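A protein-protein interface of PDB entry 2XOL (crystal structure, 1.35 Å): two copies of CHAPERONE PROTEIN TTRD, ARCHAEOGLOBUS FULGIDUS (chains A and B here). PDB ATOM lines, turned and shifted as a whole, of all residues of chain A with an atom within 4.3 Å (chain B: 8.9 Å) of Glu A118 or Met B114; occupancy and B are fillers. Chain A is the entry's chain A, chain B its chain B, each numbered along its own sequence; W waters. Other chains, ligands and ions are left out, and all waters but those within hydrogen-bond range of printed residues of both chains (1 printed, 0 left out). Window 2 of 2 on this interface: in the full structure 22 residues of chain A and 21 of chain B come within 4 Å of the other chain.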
ATOM      1  N   TYR A  81     -11.966  17.469  16.147  1.00  0.00           N
ATOM      2  CA  TYR A  81     -12.717  16.226  15.996  1.00  0.00           C
ATOM      3  C   TYR A  81     -12.462  15.569  14.644  1.00  0.00           C
ATOM      4  O   TYR A  81     -13.237  14.715  14.200  1.00  0.00           O
ATOM      5  CB  TYR A  81     -14.212  16.464  16.299  1.00  0.00           C
ATOM      6  CG  TYR A  81     -14.406  16.910  17.706  1.00  0.00           C
ATOM      7  CD1 TYR A  81     -14.443  15.982  18.736  1.00  0.00           C
ATOM      8  CD2 TYR A  81     -14.478  18.257  18.032  1.00  0.00           C
ATOM      9  CE1 TYR A  81     -14.533  16.389  20.047  1.00  0.00           C
ATOM     10  CE2 TYR A  81     -14.574  18.668  19.365  1.00  0.00           C
ATOM     11  CZ  TYR A  81     -14.606  17.720  20.368  1.00  0.00           C
ATOM     12  OH  TYR A  81     -14.654  18.104  21.701  1.00  0.00           O
ATOM     13  N   ARG A 106     -19.415   9.040  15.049  1.00  0.00           N
ATOM     14  CA  ARG A 106     -18.394   8.670  16.018  1.00  0.00           C
ATOM     15  C   ARG A 106     -19.029   8.144  17.313  1.00  0.00           C
ATOM     16  O   ARG A 106     -18.542   7.178  17.899  1.00  0.00           O
ATOM     17  CB  ARG A 106     -17.465   9.833  16.300  1.00  0.00           C
ATOM     18  CG  ARG A 106     -16.229   9.404  17.027  1.00  0.00           C
ATOM     19  CD  ARG A 106     -15.149  10.405  16.826  1.00  0.00           C
ATOM     20  NE  ARG A 106     -14.016  10.170  17.700  1.00  0.00           N
ATOM     21  CZ  ARG A 106     -13.050  11.060  17.877  1.00  0.00           C
ATOM     22  NH1 ARG A 106     -12.042  10.799  18.689  1.00  0.00           N
ATOM     23  NH2 ARG A 106     -13.121  12.218  17.247  1.00  0.00           N
ATOM     24  N   LEU A 110     -18.297   4.577  19.146  1.00  0.00           N
ATOM     25  CA  LEU A 110     -17.846   4.538  20.531  1.00  0.00           C
ATOM     26  C   LEU A 110     -18.814   3.733  21.398  1.00  0.00           C
ATOM     27  O   LEU A 110     -18.384   2.999  22.288  1.00  0.00           O
ATOM     28  CB  LEU A 110     -17.670   5.970  21.072  1.00  0.00           C
ATOM     29  CG  LEU A 110     -16.505   6.745  20.450  1.00  0.00           C
ATOM     30  CD1 LEU A 110     -16.612   8.219  20.806  1.00  0.00           C
ATOM     31  CD2 LEU A 110     -15.168   6.139  20.906  1.00  0.00           C
ATOM     32  N   LYS A 115     -16.775   2.336  24.697  1.00  0.00           N
ATOM     33  CA  LYS A 115     -15.768   3.320  25.117  1.00  0.00           C
ATOM     34  C   LYS A 115     -16.488   4.489  25.765  1.00  0.00           C
ATOM     35  O   LYS A 115     -16.818   5.486  25.113  1.00  0.00           O
ATOM     36  CB  LYS A 115     -14.904   3.784  23.944  1.00  0.00           C
ATOM     37  CG  LYS A 115     -13.953   2.730  23.422  1.00  0.00           C
ATOM     38  CD  LYS A 115     -13.136   3.250  22.246  1.00  0.00           C
ATOM     39  CE  LYS A 115     -11.941   2.350  21.950  1.00  0.00           C
ATOM     40  NZ  LYS A 115     -11.305   2.646  20.635  1.00  0.00           N
ATOM     41  N   GLU A 116     -16.742   4.362  27.058  1.00  0.00           N
ATOM     42  CA  GLU A 116     -17.638   5.266  27.776  1.00  0.00           C
ATOM     43  C   GLU A 116     -17.111   6.692  27.927  1.00  0.00           C
ATOM     44  O   GLU A 116     -17.848   7.652  27.658  1.00  0.00           O
ATOM     45  CB  GLU A 116     -17.961   4.699  29.165  1.00  0.00           C
ATOM     46  CG  GLU A 116     -19.254   5.247  29.764  1.00  0.00           C
ATOM     47  CD  GLU A 116     -20.475   4.884  28.940  1.00  0.00           C
ATOM     48  OE1 GLU A 116     -21.513   5.569  29.068  1.00  0.00           O
ATOM     49  OE2 GLU A 116     -20.397   3.906  28.161  1.00  0.00           O
ATOM     50  N   GLU A 117     -15.852   6.827  28.360  1.00  0.00           N
ATOM     51  CA  GLU A 117     -15.242   8.150  28.558  1.00  0.00           C
ATOM     52  C   GLU A 117     -15.332   8.966  27.276  1.00  0.00           C
ATOM     53  O   GLU A 117     -15.806  10.109  27.285  1.00  0.00           O
ATOM     54  CB  GLU A 117     -13.772   8.032  28.992  1.00  0.00           C
ATOM     55  CG  GLU A 117     -13.574   7.640  30.454  1.00  0.00           C
ATOM     56  CD  GLU A 117     -13.877   8.770  31.433  1.00  0.00           C
ATOM     57  OE1 GLU A 117     -14.161   9.904  30.991  1.00  0.00           O
ATOM     58  OE2 GLU A 117     -13.827   8.519  32.654  1.00  0.00           O
ATOM     59  N   GLU A 118     -14.885   8.359  26.182  1.00  0.00           N
ATOM     60  CA  GLU A 118     -14.898   9.021  24.894  1.00  0.00           C
ATOM     61  C   GLU A 118     -16.324   9.285  24.375  1.00  0.00           C
ATOM     62  O   GLU A 118     -16.589  10.344  23.858  1.00  0.00           O
ATOM     63  CB  GLU A 118     -14.077   8.229  23.882  1.00  0.00           C
ATOM     64  CG  GLU A 118     -13.463   9.069  22.777  1.00  0.00           C
ATOM     65  CD  GLU A 118     -12.521   8.272  21.898  1.00  0.00           C
ATOM     66  OE1 GLU A 118     -12.000   7.220  22.360  1.00  0.00           O
ATOM     67  OE2 GLU A 118     -12.286   8.704  20.751  1.00  0.00           O
ATOM     68  N   LEU A 119     -17.232   8.335  24.545  1.00  0.00           N
ATOM     69  CA  LEU A 119     -18.634   8.507  24.127  1.00  0.00           C
ATOM     70  C   LEU A 119     -19.297   9.757  24.753  1.00  0.00           C
ATOM     71  O   LEU A 119     -19.905  10.584  24.061  1.00  0.00           O
ATOM     72  CB  LEU A 119     -19.404   7.241  24.478  1.00  0.00           C
ATOM     73  CG  LEU A 119     -20.859   7.183  24.073  1.00  0.00           C
ATOM     74  CD1 LEU A 119     -21.753   8.135  24.829  1.00  0.00           C
ATOM     75  CD2 LEU A 119     -20.978   7.409  22.621  1.00  0.00           C
ATOM     76  N   TYR A 120     -19.113   9.925  26.060  1.00  0.00           N
ATOM     77  CA  TYR A 120     -19.641  11.071  26.803  1.00  0.00           C
ATOM     78  C   TYR A 120     -19.086  12.391  26.290  1.00  0.00           C
ATOM     79  O   TYR A 120     -19.823  13.390  26.152  1.00  0.00           O
ATOM     80  CB  TYR A 120     -19.242  10.984  28.283  1.00  0.00           C
ATOM     81  CG  TYR A 120     -19.623  12.251  29.017  1.00  0.00           C
ATOM     82  CD1 TYR A 120     -20.902  12.408  29.559  1.00  0.00           C
ATOM     83  CD2 TYR A 120     -18.735  13.327  29.104  1.00  0.00           C
ATOM     84  CE1 TYR A 120     -21.270  13.592  30.211  1.00  0.00           C
ATOM     85  CE2 TYR A 120     -19.095  14.505  29.728  1.00  0.00           C
ATOM     86  CZ  TYR A 120     -20.361  14.635  30.283  1.00  0.00           C
ATOM     87  OH  TYR A 120     -20.702  15.808  30.924  1.00  0.00           O
ATOM     88  N   LYS A 121     -17.781  12.381  26.037  1.00  0.00           N
ATOM     89  CA  LYS A 121     -17.081  13.563  25.554  1.00  0.00           C
ATOM     90  C   LYS A 121     -17.669  13.955  24.206  1.00  0.00           C
ATOM     91  O   LYS A 121     -17.895  15.133  23.949  1.00  0.00           O
ATOM     92  CB  LYS A 121     -15.568  13.331  25.404  1.00  0.00           C
ATOM     93  CG  LYS A 121     -14.765  13.271  26.731  1.00  0.00           C
ATOM     94  CD  LYS A 121     -13.335  12.832  26.454  1.00  0.00           C
ATOM     95  CE  LYS A 121     -12.438  12.840  27.707  1.00  0.00           C
ATOM     96  NZ  LYS A 121     -11.012  12.724  27.327  1.00  0.00           N
ATOM     97  N   ILE A 122     -17.923  12.961  23.355  1.00  0.00           N
ATOM     98  CA  ILE A 122     -18.418  13.248  22.006  1.00  0.00           C
ATOM     99  C   ILE A 122     -19.844  13.778  22.047  1.00  0.00           C
ATOM    100  O   ILE A 122     -20.191  14.683  21.315  1.00  0.00           O
ATOM    101  CB  ILE A 122     -18.297  12.008  21.102  1.00  0.00           C
ATOM    102  CG1 ILE A 122     -16.837  11.771  20.694  1.00  0.00           C
ATOM    103  CG2 ILE A 122     -19.161  12.134  19.860  1.00  0.00           C
ATOM    104  CD1 ILE A 122     -16.232  12.847  19.778  1.00  0.00           C
ATOM    105  N   GLU B 107      -5.814  25.494  26.710  1.00  0.00           N
ATOM    106  CA  GLU B 107      -6.782  25.207  25.657  1.00  0.00           C
ATOM    107  C   GLU B 107      -6.321  24.076  24.750  1.00  0.00           C
ATOM    108  O   GLU B 107      -7.107  23.181  24.414  1.00  0.00           O
ATOM    109  CB  GLU B 107      -7.029  26.461  24.842  1.00  0.00           C
ATOM    110  CG  GLU B 107      -7.924  26.254  23.652  1.00  0.00           C
ATOM    111  CD  GLU B 107      -8.057  27.479  22.777  1.00  0.00           C
ATOM    112  OE1 GLU B 107      -8.630  27.332  21.696  1.00  0.00           O
ATOM    113  OE2 GLU B 107      -7.583  28.580  23.143  1.00  0.00           O
ATOM    114  N   ILE B 108      -5.054  24.114  24.342  1.00  0.00           N
ATOM    115  CA  ILE B 108      -4.483  23.079  23.468  1.00  0.00           C
ATOM    116  C   ILE B 108      -4.588  21.709  24.124  1.00  0.00           C
ATOM    117  O   ILE B 108      -4.984  20.734  23.465  1.00  0.00           O
ATOM    118  CB  ILE B 108      -3.034  23.435  23.074  1.00  0.00           C
ATOM    119  CG1 ILE B 108      -3.086  24.639  22.145  1.00  0.00           C
ATOM    120  CG2 ILE B 108      -2.301  22.259  22.425  1.00  0.00           C
ATOM    121  CD1 ILE B 108      -1.740  25.272  21.885  1.00  0.00           C
ATOM    122  N   SER B 109      -4.264  21.642  25.414  1.00  0.00           N
ATOM    123  CA  SER B 109      -4.367  20.392  26.140  1.00  0.00           C
ATOM    124  C   SER B 109      -5.808  19.890  26.224  1.00  0.00           C
ATOM    125  O   SER B 109      -6.099  18.699  25.990  1.00  0.00           O
ATOM    126  CB  SER B 109      -3.769  20.523  27.546  1.00  0.00           C
ATOM    127  OG  SER B 109      -3.901  19.277  28.200  1.00  0.00           O
ATOM    128  N   LEU B 110      -6.709  20.793  26.571  1.00  0.00           N
ATOM    129  CA  LEU B 110      -8.121  20.435  26.670  1.00  0.00           C
ATOM    130  C   LEU B 110      -8.688  19.995  25.316  1.00  0.00           C
ATOM    131  O   LEU B 110      -9.518  19.084  25.260  1.00  0.00           O
ATOM    132  CB  LEU B 110      -8.923  21.586  27.251  1.00  0.00           C
ATOM    133  CG  LEU B 110      -8.568  21.996  28.680  1.00  0.00           C
ATOM    134  CD1 LEU B 110      -9.233  23.314  29.052  1.00  0.00           C
ATOM    135  CD2 LEU B 110      -8.966  20.870  29.654  1.00  0.00           C
ATOM    136  N   ALA B 111      -8.236  20.625  24.232  1.00  0.00           N
ATOM    137  CA  ALA B 111      -8.663  20.232  22.878  1.00  0.00           C
ATOM    138  C   ALA B 111      -8.214  18.800  22.559  1.00  0.00           C
ATOM    139  O   ALA B 111      -9.000  18.000  22.068  1.00  0.00           O
ATOM    140  CB  ALA B 111      -8.104  21.200  21.852  1.00  0.00           C
ATOM    141  N   GLN B 112      -6.958  18.487  22.859  1.00  0.00           N
ATOM    142  CA  GLN B 112      -6.426  17.142  22.657  1.00  0.00           C
ATOM    143  C   GLN B 112      -7.219  16.112  23.471  1.00  0.00           C
ATOM    144  O   GLN B 112      -7.437  15.004  23.001  1.00  0.00           O
ATOM    145  CB  GLN B 112      -4.928  17.116  23.036  1.00  0.00           C
ATOM    146  CG  GLN B 112      -4.050  17.886  22.031  1.00  0.00           C
ATOM    147  CD  GLN B 112      -2.624  18.235  22.496  1.00  0.00           C
ATOM    148  OE1 GLN B 112      -2.295  18.232  23.691  1.00  0.00           O
ATOM    149  NE2 GLN B 112      -1.774  18.568  21.527  1.00  0.00           N
ATOM    150  N   GLN B 113      -7.685  16.494  24.653  1.00  0.00           N
ATOM    151  CA  GLN B 113      -8.476  15.627  25.527  1.00  0.00           C
ATOM    152  C   GLN B 113      -9.974  15.606  25.184  1.00  0.00           C
ATOM    153  O   GLN B 113     -10.743  14.918  25.845  1.00  0.00           O
ATOM    154  CB  GLN B 113      -8.322  16.109  26.961  1.00  0.00           C
ATOM    155  CG  GLN B 113      -6.913  15.948  27.535  1.00  0.00           C
ATOM    156  CD  GLN B 113      -6.850  16.394  28.966  1.00  0.00           C
ATOM    157  OE1 GLN B 113      -7.344  15.704  29.860  1.00  0.00           O
ATOM    158  NE2 GLN B 113      -6.252  17.556  29.201  1.00  0.00           N
ATOM    159  N   MET B 114     -10.389  16.409  24.209  1.00  0.00           N
ATOM    160  CA  MET B 114     -11.811  16.534  23.823  1.00  0.00           C
ATOM    161  C   MET B 114     -12.678  16.905  25.036  1.00  0.00           C
ATOM    162  O   MET B 114     -13.779  16.398  25.214  1.00  0.00           O
ATOM    163  CB  MET B 114     -12.311  15.271  23.101  1.00  0.00           C
ATOM    164  CG  MET B 114     -11.571  15.004  21.808  1.00  0.00           C
ATOM    165  SD  MET B 114     -12.191  13.567  20.910  1.00  0.00           S
ATOM    166  CE  MET B 114     -11.779  12.243  22.031  1.00  0.00           C
ATOM    167  N   LYS B 115     -12.138  17.793  25.878  1.00  0.00           N
ATOM    168  CA  LYS B 115     -12.849  18.353  27.033  1.00  0.00           C
ATOM    169  C   LYS B 115     -13.501  19.673  26.637  1.00  0.00           C
ATOM    170  O   LYS B 115     -13.016  20.770  26.925  1.00  0.00           O
ATOM    171  CB  LYS B 115     -11.907  18.516  28.224  1.00  0.00           C
ATOM    172  CG  LYS B 115     -11.605  17.203  28.911  1.00  0.00           C
ATOM    173  CD  LYS B 115     -10.552  17.373  30.008  1.00  0.00           C
ATOM    174  CE  LYS B 115     -10.346  16.123  30.847  1.00  0.00           C
ATOM    175  NZ  LYS B 115      -9.175  16.243  31.793  1.00  0.00           N
ATOM    176  N   GLU B 116     -14.614  19.559  25.924  1.00  0.00           N
ATOM    177  CA  GLU B 116     -15.217  20.726  25.286  1.00  0.00           C
ATOM    178  C   GLU B 116     -15.785  21.763  26.268  1.00  0.00           C
ATOM    179  O   GLU B 116     -15.606  22.948  26.081  1.00  0.00           O
ATOM    180  CB  GLU B 116     -16.285  20.252  24.294  1.00  0.00           C
ATOM    181  CG  GLU B 116     -16.599  21.222  23.239  1.00  0.00           C
ATOM    182  CD  GLU B 116     -15.422  21.599  22.352  1.00  0.00           C
ATOM    183  OE1 GLU B 116     -15.375  22.794  22.065  1.00  0.00           O
ATOM    184  OE2 GLU B 116     -14.576  20.748  21.939  1.00  0.00           O
ATOM    185  N   GLU B 117     -16.466  21.325  27.325  1.00  0.00           N
ATOM    186  CA  GLU B 117     -17.015  22.278  28.287  1.00  0.00           C
ATOM    187  C   GLU B 117     -15.890  23.024  29.039  1.00  0.00           C
ATOM    188  O   GLU B 117     -15.980  24.233  29.252  1.00  0.00           O
ATOM    189  CB  GLU B 117     -17.972  21.591  29.286  1.00  0.00           C
ATOM    190  CG  GLU B 117     -19.291  21.176  28.644  1.00  0.00           C
ATOM    191  CD  GLU B 117     -20.113  22.366  28.175  1.00  0.00           C
ATOM    192  OE1 GLU B 117     -20.260  23.358  28.921  1.00  0.00           O
ATOM    193  OE2 GLU B 117     -20.630  22.304  27.043  1.00  0.00           O
ATOM    194  N   GLU B 118     -14.825  22.317  29.396  1.00  0.00           N
ATOM    195  CA  GLU B 118     -13.710  22.982  30.058  1.00  0.00           C
ATOM    196  C   GLU B 118     -12.962  23.900  29.085  1.00  0.00           C
ATOM    197  O   GLU B 118     -12.544  24.988  29.469  1.00  0.00           O
ATOM    198  CB  GLU B 118     -12.776  21.988  30.714  1.00  0.00           C
ATOM    199  CG  GLU B 118     -11.936  22.649  31.808  1.00  0.00           C
ATOM    200  CD  GLU B 118     -11.039  21.695  32.569  1.00  0.00           C
ATOM    201  OE1 GLU B 118     -11.245  20.463  32.486  1.00  0.00           O
ATOM    202  OE2 GLU B 118     -10.101  22.185  33.248  1.00  0.00           O
ATOM    203  N   LEU B 119     -12.851  23.487  27.819  1.00  0.00           N
ATOM    204  CA  LEU B 119     -12.214  24.333  26.802  1.00  0.00           C
ATOM    205  C   LEU B 119     -13.011  25.634  26.660  1.00  0.00           C
ATOM    206  O   LEU B 119     -12.444  26.720  26.567  1.00  0.00           O
ATOM    207  CB  LEU B 119     -12.128  23.589  25.474  1.00  0.00           C
ATOM    208  CG  LEU B 119     -11.391  24.279  24.321  1.00  0.00           C
ATOM    209  CD1 LEU B 119     -10.763  23.261  23.361  1.00  0.00           C
ATOM    210  CD2 LEU B 119     -12.277  25.262  23.555  1.00  0.00           C
HETATM  211  O   HOH W   1     -16.327  16.912  25.468  1.00  0.00           O
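Of the printed residues of chain A, Met B114 touches Tyr A81, Arg A106, Glu A118 and Lys A121.
Printed residues of chain B within 4 Å of Lys A121: Gln B113 and Met B114.
Of the printed residues of chain B, Tyr A81 touches Met B114 and Glu B116.
The nearest residue of chain B that does not touch Glu A118 is Gln B113 (7.1 Å).
The nearest printed residue of chain A that does not touch Met B114 is Ile A122 (4.3 Å).
Of the 13 printed residues of chain B, 3 touch a printed residue of chain A.
Hydrophobic or aromatic side chains of chain B that line the printed part of chain A: Met B114.
Of the 11 printed residues of chain A, 4 touch a printed residue of chain B.
Among the printed residues, 6 pairs touch across the chains.
Positions printed for both chains: 110, 115, 116, 117, 118 and 119.
NH1 of Arg A106 lies within salt-bridge range of OE2 of Glu A118 (2.9 Å).
OG of Ser B109 lies within hydrogen-bond range of NE2 of Gln B113 (3.1 Å).
The side-chain amino group of Lys B115 lies within hydrogen-bond range of the side-chain amide oxygen of Gln B113 (2.7 Å).
Water W1 lies within hydrogen-bond range of O of Met B114 (2.6 Å), O of Lys A121 (2.8 Å) and N of Glu B116 (3.2 Å).
Among the printed residues, merely in contact across the chains: Tyr A81 with Met B114, Glu A118 with Met B114 and Lys A121 with Met B114.
OH of Tyr A81 sits at hydrogen-bond distance from OE2 of Glu B116 (2.7 Å).
NH1 of Arg A106 lies within hydrogen-bond range of SD of Met B114.
O of Gln B113 is in hydrogen-bond range of NZ of Lys A121.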
